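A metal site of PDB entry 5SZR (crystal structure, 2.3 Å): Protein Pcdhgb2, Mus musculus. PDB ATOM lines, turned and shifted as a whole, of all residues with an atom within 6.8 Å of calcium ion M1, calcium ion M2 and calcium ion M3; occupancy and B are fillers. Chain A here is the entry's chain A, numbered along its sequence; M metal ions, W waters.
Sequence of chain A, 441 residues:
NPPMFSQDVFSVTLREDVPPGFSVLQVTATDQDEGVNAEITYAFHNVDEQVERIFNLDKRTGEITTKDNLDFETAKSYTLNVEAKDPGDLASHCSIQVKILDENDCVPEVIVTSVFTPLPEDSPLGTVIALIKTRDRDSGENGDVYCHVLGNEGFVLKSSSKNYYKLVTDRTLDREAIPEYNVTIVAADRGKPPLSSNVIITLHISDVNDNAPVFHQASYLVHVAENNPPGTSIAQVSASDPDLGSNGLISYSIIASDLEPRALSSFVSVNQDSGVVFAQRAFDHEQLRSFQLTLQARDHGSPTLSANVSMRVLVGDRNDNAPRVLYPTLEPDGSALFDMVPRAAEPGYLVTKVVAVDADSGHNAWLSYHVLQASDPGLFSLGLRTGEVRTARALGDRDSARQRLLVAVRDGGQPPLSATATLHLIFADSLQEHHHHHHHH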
ATOM      1  N   GLU A 121     -18.269  21.369 -27.786  1.00  0.00           N
ATOM      2  CA  GLU A 121     -17.191  20.627 -28.434  1.00  0.00           C
ATOM      3  C   GLU A 121     -16.795  19.361 -27.683  1.00  0.00           C
ATOM      4  O   GLU A 121     -16.124  18.503 -28.253  1.00  0.00           O
ATOM      5  CB  GLU A 121     -15.964  21.531 -28.590  1.00  0.00           C
ATOM      6  CG  GLU A 121     -15.275  21.876 -27.280  1.00  0.00           C
ATOM      7  CD  GLU A 121     -14.039  22.710 -27.496  1.00  0.00           C
ATOM      8  OE1 GLU A 121     -13.826  23.666 -26.719  1.00  0.00           O
ATOM      9  OE2 GLU A 121     -13.282  22.433 -28.447  1.00  0.00           O
ATOM     10  N   LEU A 173     -15.486  16.209 -31.243  1.00  0.00           N
ATOM     11  CA  LEU A 173     -15.458  17.527 -31.846  1.00  0.00           C
ATOM     12  C   LEU A 173     -14.299  18.346 -31.281  1.00  0.00           C
ATOM     13  O   LEU A 173     -13.669  17.978 -30.281  1.00  0.00           O
ATOM     14  CB  LEU A 173     -16.785  18.236 -31.612  1.00  0.00           C
ATOM     15  CG  LEU A 173     -17.990  17.470 -32.199  1.00  0.00           C
ATOM     16  CD1 LEU A 173     -19.293  17.925 -31.560  1.00  0.00           C
ATOM     17  CD2 LEU A 173     -18.046  17.641 -33.706  1.00  0.00           C
ATOM     18  N   ASP A 174     -14.006  19.467 -31.943  1.00  0.00           N
ATOM     19  CA  ASP A 174     -12.928  20.343 -31.503  1.00  0.00           C
ATOM     20  C   ASP A 174     -13.182  21.717 -32.108  1.00  0.00           C
ATOM     21  O   ASP A 174     -12.954  21.922 -33.297  1.00  0.00           O
ATOM     22  CB  ASP A 174     -11.561  19.793 -31.914  1.00  0.00           C
ATOM     23  CG  ASP A 174     -10.411  20.690 -31.472  1.00  0.00           C
ATOM     24  OD1 ASP A 174     -10.631  21.580 -30.626  1.00  0.00           O
ATOM     25  OD2 ASP A 174      -9.285  20.492 -31.961  1.00  0.00           O
ATOM     26  N   ARG A 175     -13.633  22.662 -31.273  1.00  0.00           N
ATOM     27  CA  ARG A 175     -13.918  24.010 -31.748  1.00  0.00           C
ATOM     28  C   ARG A 175     -12.665  24.661 -32.316  1.00  0.00           C
ATOM     29  O   ARG A 175     -12.748  25.401 -33.310  1.00  0.00           O
ATOM     30  CB  ARG A 175     -14.493  24.864 -30.616  1.00  0.00           C
ATOM     31  CG  ARG A 175     -15.027  26.196 -31.093  1.00  0.00           C
ATOM     32  CD  ARG A 175     -15.077  27.214 -29.974  1.00  0.00           C
ATOM     33  NE  ARG A 175     -13.733  27.627 -29.556  1.00  0.00           N
ATOM     34  CZ  ARG A 175     -13.033  28.593 -30.146  1.00  0.00           C
ATOM     35  NH1 ARG A 175     -13.550  29.240 -31.172  1.00  0.00           N
ATOM     36  NH2 ARG A 175     -11.823  28.900 -29.709  1.00  0.00           N
ATOM     37  N   GLU A 176     -11.513  24.415 -31.698  1.00  0.00           N
ATOM     38  CA  GLU A 176     -10.276  25.045 -32.159  1.00  0.00           C
ATOM     39  C   GLU A 176      -9.883  24.604 -33.561  1.00  0.00           C
ATOM     40  O   GLU A 176      -9.125  25.313 -34.227  1.00  0.00           O
ATOM     41  CB  GLU A 176      -9.152  24.763 -31.158  1.00  0.00           C
ATOM     42  CG  GLU A 176      -9.182  25.646 -29.901  1.00  0.00           C
ATOM     43  CD  GLU A 176     -10.301  25.288 -28.934  1.00  0.00           C
ATOM     44  OE1 GLU A 176     -10.539  24.077 -28.711  1.00  0.00           O
ATOM     45  OE2 GLU A 176     -10.946  26.210 -28.395  1.00  0.00           O
ATOM     46  N   ALA A 177     -10.382  23.459 -34.030  1.00  0.00           N
ATOM     47  CA  ALA A 177     -10.122  22.983 -35.383  1.00  0.00           C
ATOM     48  C   ALA A 177     -11.237  23.330 -36.358  1.00  0.00           C
ATOM     49  O   ALA A 177     -10.968  23.866 -37.440  1.00  0.00           O
ATOM     50  CB  ALA A 177      -9.868  21.472 -35.377  1.00  0.00           C
ATOM     51  N   SER A 206     -19.659  25.268 -29.558  1.00  0.00           N
ATOM     52  CA  SER A 206     -19.343  26.173 -28.458  1.00  0.00           C
ATOM     53  C   SER A 206     -18.065  25.727 -27.744  1.00  0.00           C
ATOM     54  O   SER A 206     -17.648  24.569 -27.814  1.00  0.00           O
ATOM     55  CB  SER A 206     -20.504  26.234 -27.460  1.00  0.00           C
ATOM     56  OG  SER A 206     -20.807  24.960 -26.946  1.00  0.00           O
ATOM     57  N   ASP A 207     -17.442  26.671 -27.051  1.00  0.00           N
ATOM     58  CA  ASP A 207     -16.098  26.470 -26.508  1.00  0.00           C
ATOM     59  C   ASP A 207     -16.138  25.832 -25.128  1.00  0.00           C
ATOM     60  O   ASP A 207     -17.049  26.083 -24.322  1.00  0.00           O
ATOM     61  CB  ASP A 207     -15.337  27.794 -26.433  1.00  0.00           C
ATOM     62  CG  ASP A 207     -13.904  27.623 -25.937  1.00  0.00           C
ATOM     63  OD1 ASP A 207     -13.119  26.925 -26.616  1.00  0.00           O
ATOM     64  OD2 ASP A 207     -13.563  28.202 -24.887  1.00  0.00           O
ATOM     65  N   VAL A 208     -15.135  24.995 -24.861  1.00  0.00           N
ATOM     66  CA  VAL A 208     -14.855  24.421 -23.551  1.00  0.00           C
ATOM     67  C   VAL A 208     -13.402  24.761 -23.225  1.00  0.00           C
ATOM     68  O   VAL A 208     -12.572  24.926 -24.125  1.00  0.00           O
ATOM     69  CB  VAL A 208     -15.098  22.894 -23.546  1.00  0.00           C
ATOM     70  CG1 VAL A 208     -14.584  22.240 -22.279  1.00  0.00           C
ATOM     71  CG2 VAL A 208     -16.588  22.611 -23.712  1.00  0.00           C
ATOM     72  N   ASN A 209     -13.103  24.927 -21.932  1.00  0.00           N
ATOM     73  CA  ASN A 209     -11.743  25.237 -21.504  1.00  0.00           C
ATOM     74  C   ASN A 209     -10.931  23.945 -21.523  1.00  0.00           C
ATOM     75  O   ASN A 209     -10.706  23.294 -20.491  1.00  0.00           O
ATOM     76  CB  ASN A 209     -11.727  25.883 -20.128  1.00  0.00           C
ATOM     77  CG  ASN A 209     -10.350  26.390 -19.738  1.00  0.00           C
ATOM     78  OD1 ASN A 209      -9.523  26.695 -20.606  1.00  0.00           O
ATOM     79  ND2 ASN A 209     -10.096  26.492 -18.445  1.00  0.00           N
ATOM     80  N   ASP A 210     -10.466  23.572 -22.713  1.00  0.00           N
ATOM     81  CA  ASP A 210      -9.648  22.372 -22.868  1.00  0.00           C
ATOM     82  C   ASP A 210      -8.237  22.681 -23.371  1.00  0.00           C
ATOM     83  O   ASP A 210      -7.547  21.778 -23.840  1.00  0.00           O
ATOM     84  CB  ASP A 210     -10.342  21.366 -23.797  1.00  0.00           C
ATOM     85  CG  ASP A 210     -10.739  21.979 -25.138  1.00  0.00           C
ATOM     86  OD1 ASP A 210     -10.821  23.226 -25.229  1.00  0.00           O
ATOM     87  OD2 ASP A 210     -10.989  21.207 -26.090  1.00  0.00           O
ATOM     88  N   ASN A 211      -7.793  23.934 -23.277  1.00  0.00           N
ATOM     89  CA  ASN A 211      -6.455  24.324 -23.703  1.00  0.00           C
ATOM     90  C   ASN A 211      -5.769  25.100 -22.595  1.00  0.00           C
ATOM     91  O   ASN A 211      -6.274  26.126 -22.150  1.00  0.00           O
ATOM     92  CB  ASN A 211      -6.499  25.163 -24.983  1.00  0.00           C
ATOM     93  CG  ASN A 211      -6.873  24.342 -26.205  1.00  0.00           C
ATOM     94  OD1 ASN A 211      -6.006  23.699 -26.816  1.00  0.00           O
ATOM     95  ND2 ASN A 211      -8.145  24.363 -26.564  1.00  0.00           N
ATOM     96  N   ALA A 212      -4.622  24.601 -22.157  1.00  0.00           N
ATOM     97  CA  ALA A 212      -3.832  25.307 -21.156  1.00  0.00           C
ATOM     98  C   ALA A 212      -3.015  26.409 -21.822  1.00  0.00           C
ATOM     99  O   ALA A 212      -2.572  26.241 -22.974  1.00  0.00           O
ATOM    100  CB  ALA A 212      -2.904  24.337 -20.425  1.00  0.00           C
ATOM    101  N   PRO A 213      -2.821  27.543 -21.166  1.00  0.00           N
ATOM    102  CA  PRO A 213      -1.923  28.564 -21.705  1.00  0.00           C
ATOM    103  C   PRO A 213      -0.532  27.997 -21.955  1.00  0.00           C
ATOM    104  O   PRO A 213      -0.081  27.079 -21.268  1.00  0.00           O
ATOM    105  CB  PRO A 213      -1.903  29.652 -20.621  1.00  0.00           C
ATOM    106  CG  PRO A 213      -2.520  29.017 -19.407  1.00  0.00           C
ATOM    107  CD  PRO A 213      -3.465  27.980 -19.915  1.00  0.00           C
ATOM    108  N   ASP A 241      -3.444  31.216 -25.591  1.00  0.00           N
ATOM    109  CA  ASP A 241      -4.510  30.297 -25.213  1.00  0.00           C
ATOM    110  C   ASP A 241      -5.626  30.368 -26.247  1.00  0.00           C
ATOM    111  O   ASP A 241      -6.313  31.397 -26.346  1.00  0.00           O
ATOM    112  CB  ASP A 241      -5.027  30.648 -23.818  1.00  0.00           C
ATOM    113  CG  ASP A 241      -5.924  29.574 -23.218  1.00  0.00           C
ATOM    114  OD1 ASP A 241      -6.875  29.134 -23.883  1.00  0.00           O
ATOM    115  OD2 ASP A 241      -5.675  29.174 -22.064  1.00  0.00           O
ATOM    116  N   PRO A 242      -5.842  29.310 -27.044  1.00  0.00           N
ATOM    117  CA  PRO A 242      -6.795  29.410 -28.161  1.00  0.00           C
ATOM    118  C   PRO A 242      -8.252  29.384 -27.742  1.00  0.00           C
ATOM    119  O   PRO A 242      -9.119  29.616 -28.591  1.00  0.00           O
ATOM    120  CB  PRO A 242      -6.455  28.180 -29.002  1.00  0.00           C
ATOM    121  CG  PRO A 242      -5.992  27.183 -28.017  1.00  0.00           C
ATOM    122  CD  PRO A 242      -5.232  27.973 -26.959  1.00  0.00           C
ATOM    123  N   ASP A 243      -8.551  29.124 -26.473  1.00  0.00           N
ATOM    124  CA  ASP A 243      -9.934  29.071 -26.017  1.00  0.00           C
ATOM    125  C   ASP A 243     -10.567  30.469 -26.054  1.00  0.00           C
ATOM    126  O   ASP A 243      -9.891  31.482 -26.261  1.00  0.00           O
ATOM    127  CB  ASP A 243     -10.009  28.458 -24.613  1.00  0.00           C
ATOM    128  CG  ASP A 243      -9.477  27.032 -24.573  1.00  0.00           C
ATOM    129  OD1 ASP A 243      -9.562  26.331 -25.606  1.00  0.00           O
ATOM    130  OD2 ASP A 243      -8.974  26.609 -23.515  1.00  0.00           O
ATOM    131  N   LEU A 244     -11.879  30.515 -25.836  1.00  0.00           N
ATOM    132  CA  LEU A 244     -12.651  31.736 -26.020  1.00  0.00           C
ATOM    133  C   LEU A 244     -12.978  32.406 -24.688  1.00  0.00           C
ATOM    134  O   LEU A 244     -13.178  31.751 -23.665  1.00  0.00           O
ATOM    135  CB  LEU A 244     -13.959  31.445 -26.758  1.00  0.00           C
ATOM    136  CG  LEU A 244     -13.927  31.329 -28.282  1.00  0.00           C
ATOM    137  CD1 LEU A 244     -15.346  31.140 -28.808  1.00  0.00           C
ATOM    138  CD2 LEU A 244     -13.257  32.539 -28.909  1.00  0.00           C
ATOM    139  N   SER A 246     -13.454  33.928 -21.255  1.00  0.00           N
ATOM    140  CA  SER A 246     -12.833  33.655 -19.966  1.00  0.00           C
ATOM    141  C   SER A 246     -11.893  32.462 -20.026  1.00  0.00           C
ATOM    142  O   SER A 246     -10.920  32.405 -19.271  1.00  0.00           O
ATOM    143  CB  SER A 246     -13.904  33.428 -18.898  1.00  0.00           C
ATOM    144  OG  SER A 246     -14.324  34.657 -18.330  1.00  0.00           O
ATOM    145  N   ASN A 247     -12.155  31.500 -20.916  1.00  0.00           N
ATOM    146  CA  ASN A 247     -11.281  30.344 -21.033  1.00  0.00           C
ATOM    147  C   ASN A 247      -9.938  30.676 -21.666  1.00  0.00           C
ATOM    148  O   ASN A 247      -9.012  29.859 -21.606  1.00  0.00           O
ATOM    149  CB  ASN A 247     -11.974  29.248 -21.837  1.00  0.00           C
ATOM    150  CG  ASN A 247     -13.273  28.786 -21.206  1.00  0.00           C
ATOM    151  OD1 ASN A 247     -13.492  28.957 -20.011  1.00  0.00           O
ATOM    152  ND2 ASN A 247     -14.142  28.202 -22.014  1.00  0.00           N
ATOM    153  N   GLY A 248      -9.801  31.853 -22.288  1.00  0.00           N
ATOM    154  CA  GLY A 248      -8.557  32.242 -22.901  1.00  0.00           C
ATOM    155  C   GLY A 248      -7.967  33.515 -22.344  1.00  0.00           C
ATOM    156  O   GLY A 248      -7.023  34.080 -22.908  1.00  0.00           O
ATOM    157  N   LEU A 249      -8.501  33.986 -21.219  1.00  0.00           N
ATOM    158  CA  LEU A 249      -8.001  35.185 -20.546  1.00  0.00           C
ATOM    159  C   LEU A 249      -6.879  34.772 -19.596  1.00  0.00           C
ATOM    160  O   LEU A 249      -7.091  33.960 -18.699  1.00  0.00           O
ATOM    161  CB  LEU A 249      -9.124  35.883 -19.790  1.00  0.00           C
ATOM    162  CG  LEU A 249      -8.799  37.235 -19.150  1.00  0.00           C
ATOM    163  CD1 LEU A 249      -8.405  38.251 -20.206  1.00  0.00           C
ATOM    164  CD2 LEU A 249      -9.971  37.743 -18.323  1.00  0.00           C
ATOM    165  N   ILE A 250      -5.691  35.360 -19.786  1.00  0.00           N
ATOM    166  CA  ILE A 250      -4.482  34.941 -19.081  1.00  0.00           C
ATOM    167  C   ILE A 250      -4.175  35.890 -17.935  1.00  0.00           C
ATOM    168  O   ILE A 250      -4.297  37.117 -18.066  1.00  0.00           O
ATOM    169  CB  ILE A 250      -3.275  34.871 -20.039  1.00  0.00           C
ATOM    170  CG1 ILE A 250      -3.608  34.022 -21.271  1.00  0.00           C
ATOM    171  CG2 ILE A 250      -2.058  34.304 -19.330  1.00  0.00           C
ATOM    172  CD1 ILE A 250      -3.920  32.600 -20.929  1.00  0.00           C
ATOM    173  N   ASP A 299      -5.343  30.540 -16.990  1.00  0.00           N
ATOM    174  CA  ASP A 299      -6.546  31.046 -17.631  1.00  0.00           C
ATOM    175  C   ASP A 299      -7.670  31.188 -16.602  1.00  0.00           C
ATOM    176  O   ASP A 299      -7.542  30.774 -15.447  1.00  0.00           O
ATOM    177  CB  ASP A 299      -6.967  30.175 -18.825  1.00  0.00           C
ATOM    178  CG  ASP A 299      -7.453  28.770 -18.427  1.00  0.00           C
ATOM    179  OD1 ASP A 299      -8.034  28.580 -17.350  1.00  0.00           O
ATOM    180  OD2 ASP A 299      -7.250  27.852 -19.246  1.00  0.00           O
ATOM    181  N   HIS A 300      -8.778  31.789 -17.029  1.00  0.00           N
ATOM    182  CA  HIS A 300      -9.921  32.046 -16.157  1.00  0.00           C
ATOM    183  C   HIS A 300     -11.118  31.163 -16.517  1.00  0.00           C
ATOM    184  O   HIS A 300     -12.260  31.624 -16.540  1.00  0.00           O
ATOM    185  CB  HIS A 300     -10.302  33.519 -16.189  1.00  0.00           C
ATOM    186  CG  HIS A 300      -9.309  34.420 -15.541  1.00  0.00           C
ATOM    187  ND1 HIS A 300      -9.148  34.480 -14.172  1.00  0.00           N
ATOM    188  CD2 HIS A 300      -8.412  35.290 -16.064  1.00  0.00           C
ATOM    189  CE1 HIS A 300      -8.202  35.359 -13.875  1.00  0.00           C
ATOM    190  NE2 HIS A 300      -7.739  35.858 -15.004  1.00  0.00           N
ATOM    191  N   GLY A 301     -10.855  29.880 -16.795  1.00  0.00           N
ATOM    192  CA  GLY A 301     -11.907  28.920 -17.058  1.00  0.00           C
ATOM    193  C   GLY A 301     -12.249  28.091 -15.827  1.00  0.00           C
ATOM    194  O   GLY A 301     -11.645  28.195 -14.768  1.00  0.00           O
ATOM    195  N   LEU A 305      -6.752  26.281 -16.189  1.00  0.00           N
ATOM    196  CA  LEU A 305      -5.566  25.617 -16.712  1.00  0.00           C
ATOM    197  C   LEU A 305      -4.389  26.579 -16.623  1.00  0.00           C
ATOM    198  O   LEU A 305      -4.564  27.803 -16.617  1.00  0.00           O
ATOM    199  CB  LEU A 305      -5.796  25.155 -18.151  1.00  0.00           C
ATOM    200  CG  LEU A 305      -6.844  24.049 -18.247  1.00  0.00           C
ATOM    201  CD1 LEU A 305      -7.228  23.795 -19.702  1.00  0.00           C
ATOM    202  CD2 LEU A 305      -6.327  22.778 -17.604  1.00  0.00           C
HETATM  203 CA    CA M   1      -7.806  27.869 -21.809  1.00  0.00          CA
HETATM  204 CA    CA M   2     -11.649  25.143 -26.318  1.00  0.00          CA
HETATM  205 CA    CA M   3     -10.925  21.828 -28.320  1.00  0.00          CA
HETATM  206  O   HOH W   1      -8.423  21.624 -28.217  1.00  0.00           O
HETATM  207  O   HOH W   2     -11.107  19.471 -28.677  1.00  0.00           O
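Calcium ion M1 is bound by O of Asn 247, O of Asn 211, OD1 of Asn 209, OD2 of Asp 243, OD2 of Asp 241, OD1 of Asp 241 and OD2 of Asp 299.
Four residues have an atom within 4 Å of calcium ion M3: Glu 121, Asp 174, Glu 176 and Asp 210.
The nearest printed residue that does not touch calcium ion M3 is Arg 175 (4.1 Å).
Along chain A the residues within 4 Å of calcium ion M2 span positions 121 to 243.
OD2 of Asp 207 sits at hydrogen-bond distance from N of Leu 244 (3.0 Å).
The side-chain carboxylate (OD1) of Asp 299 lies within hydrogen-bond range of the backbone NH (N) of Gly 301, 3.2 Å away.
The side-chain amide nitrogen (ND2) of Asn 211 lies close to the side-chain carboxylate (OE1) of Glu 176 (3.2 Å).
The backbone NH (N) of Glu 121 lies within hydrogen-bond range of the backbone carbonyl oxygen (O) of Ser 206 (3.3 Å).
The side-chain carboxylate (OD2) of Asp 207 lies within hydrogen-bond range of the side-chain amide nitrogen (ND2) of Asn 247.
O of Leu 305 is in hydrogen-bond range of N of Asp 299.
The side-chain amide nitrogen of Asn 211 sits close to the side-chain carboxylate of Asp 210 (3.2 Å).
The side-chain carboxylate of Asp 207 lies close to the guanidinium group of Arg 175, at 3.1 Å.
The side-chain carboxylate (OD1) of Asp 207 is bound to calcium ion M2.
OD1 of Asp 210 binds calcium ion M2, at 2.4 Å.
Calcium ion M2 is bound by O of Val 208 (2.4 Å).
OE2 of Glu 176 binds calcium ion M2 (2.4 Å).
The side-chain carboxylate (OD1) of Asp 243 binds calcium ion M2.
OE1 of Glu 121 is bound to calcium ion M2.
Calcium ion M2 is bound by the side-chain carboxylate (OE1) of Glu 176 (2.8 Å).
Calcium ion M2 has seven donor atoms within binding distance.
Calcium ion M3 is bound by the side-chain carboxylate of Glu 176 (2.3 Å), the side-chain carboxylate of Asp 210 (2.3 Å), the side-chain carboxylate of Asp 174 (2.3 Å), water W2 (2.4 Å), the side-chain carboxylate of Glu 121 (2.4 Å) and water W1 (2.5 Å).
The nearest printed residue that does not touch calcium ion M1 is Gly 248 (4.5 Å).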
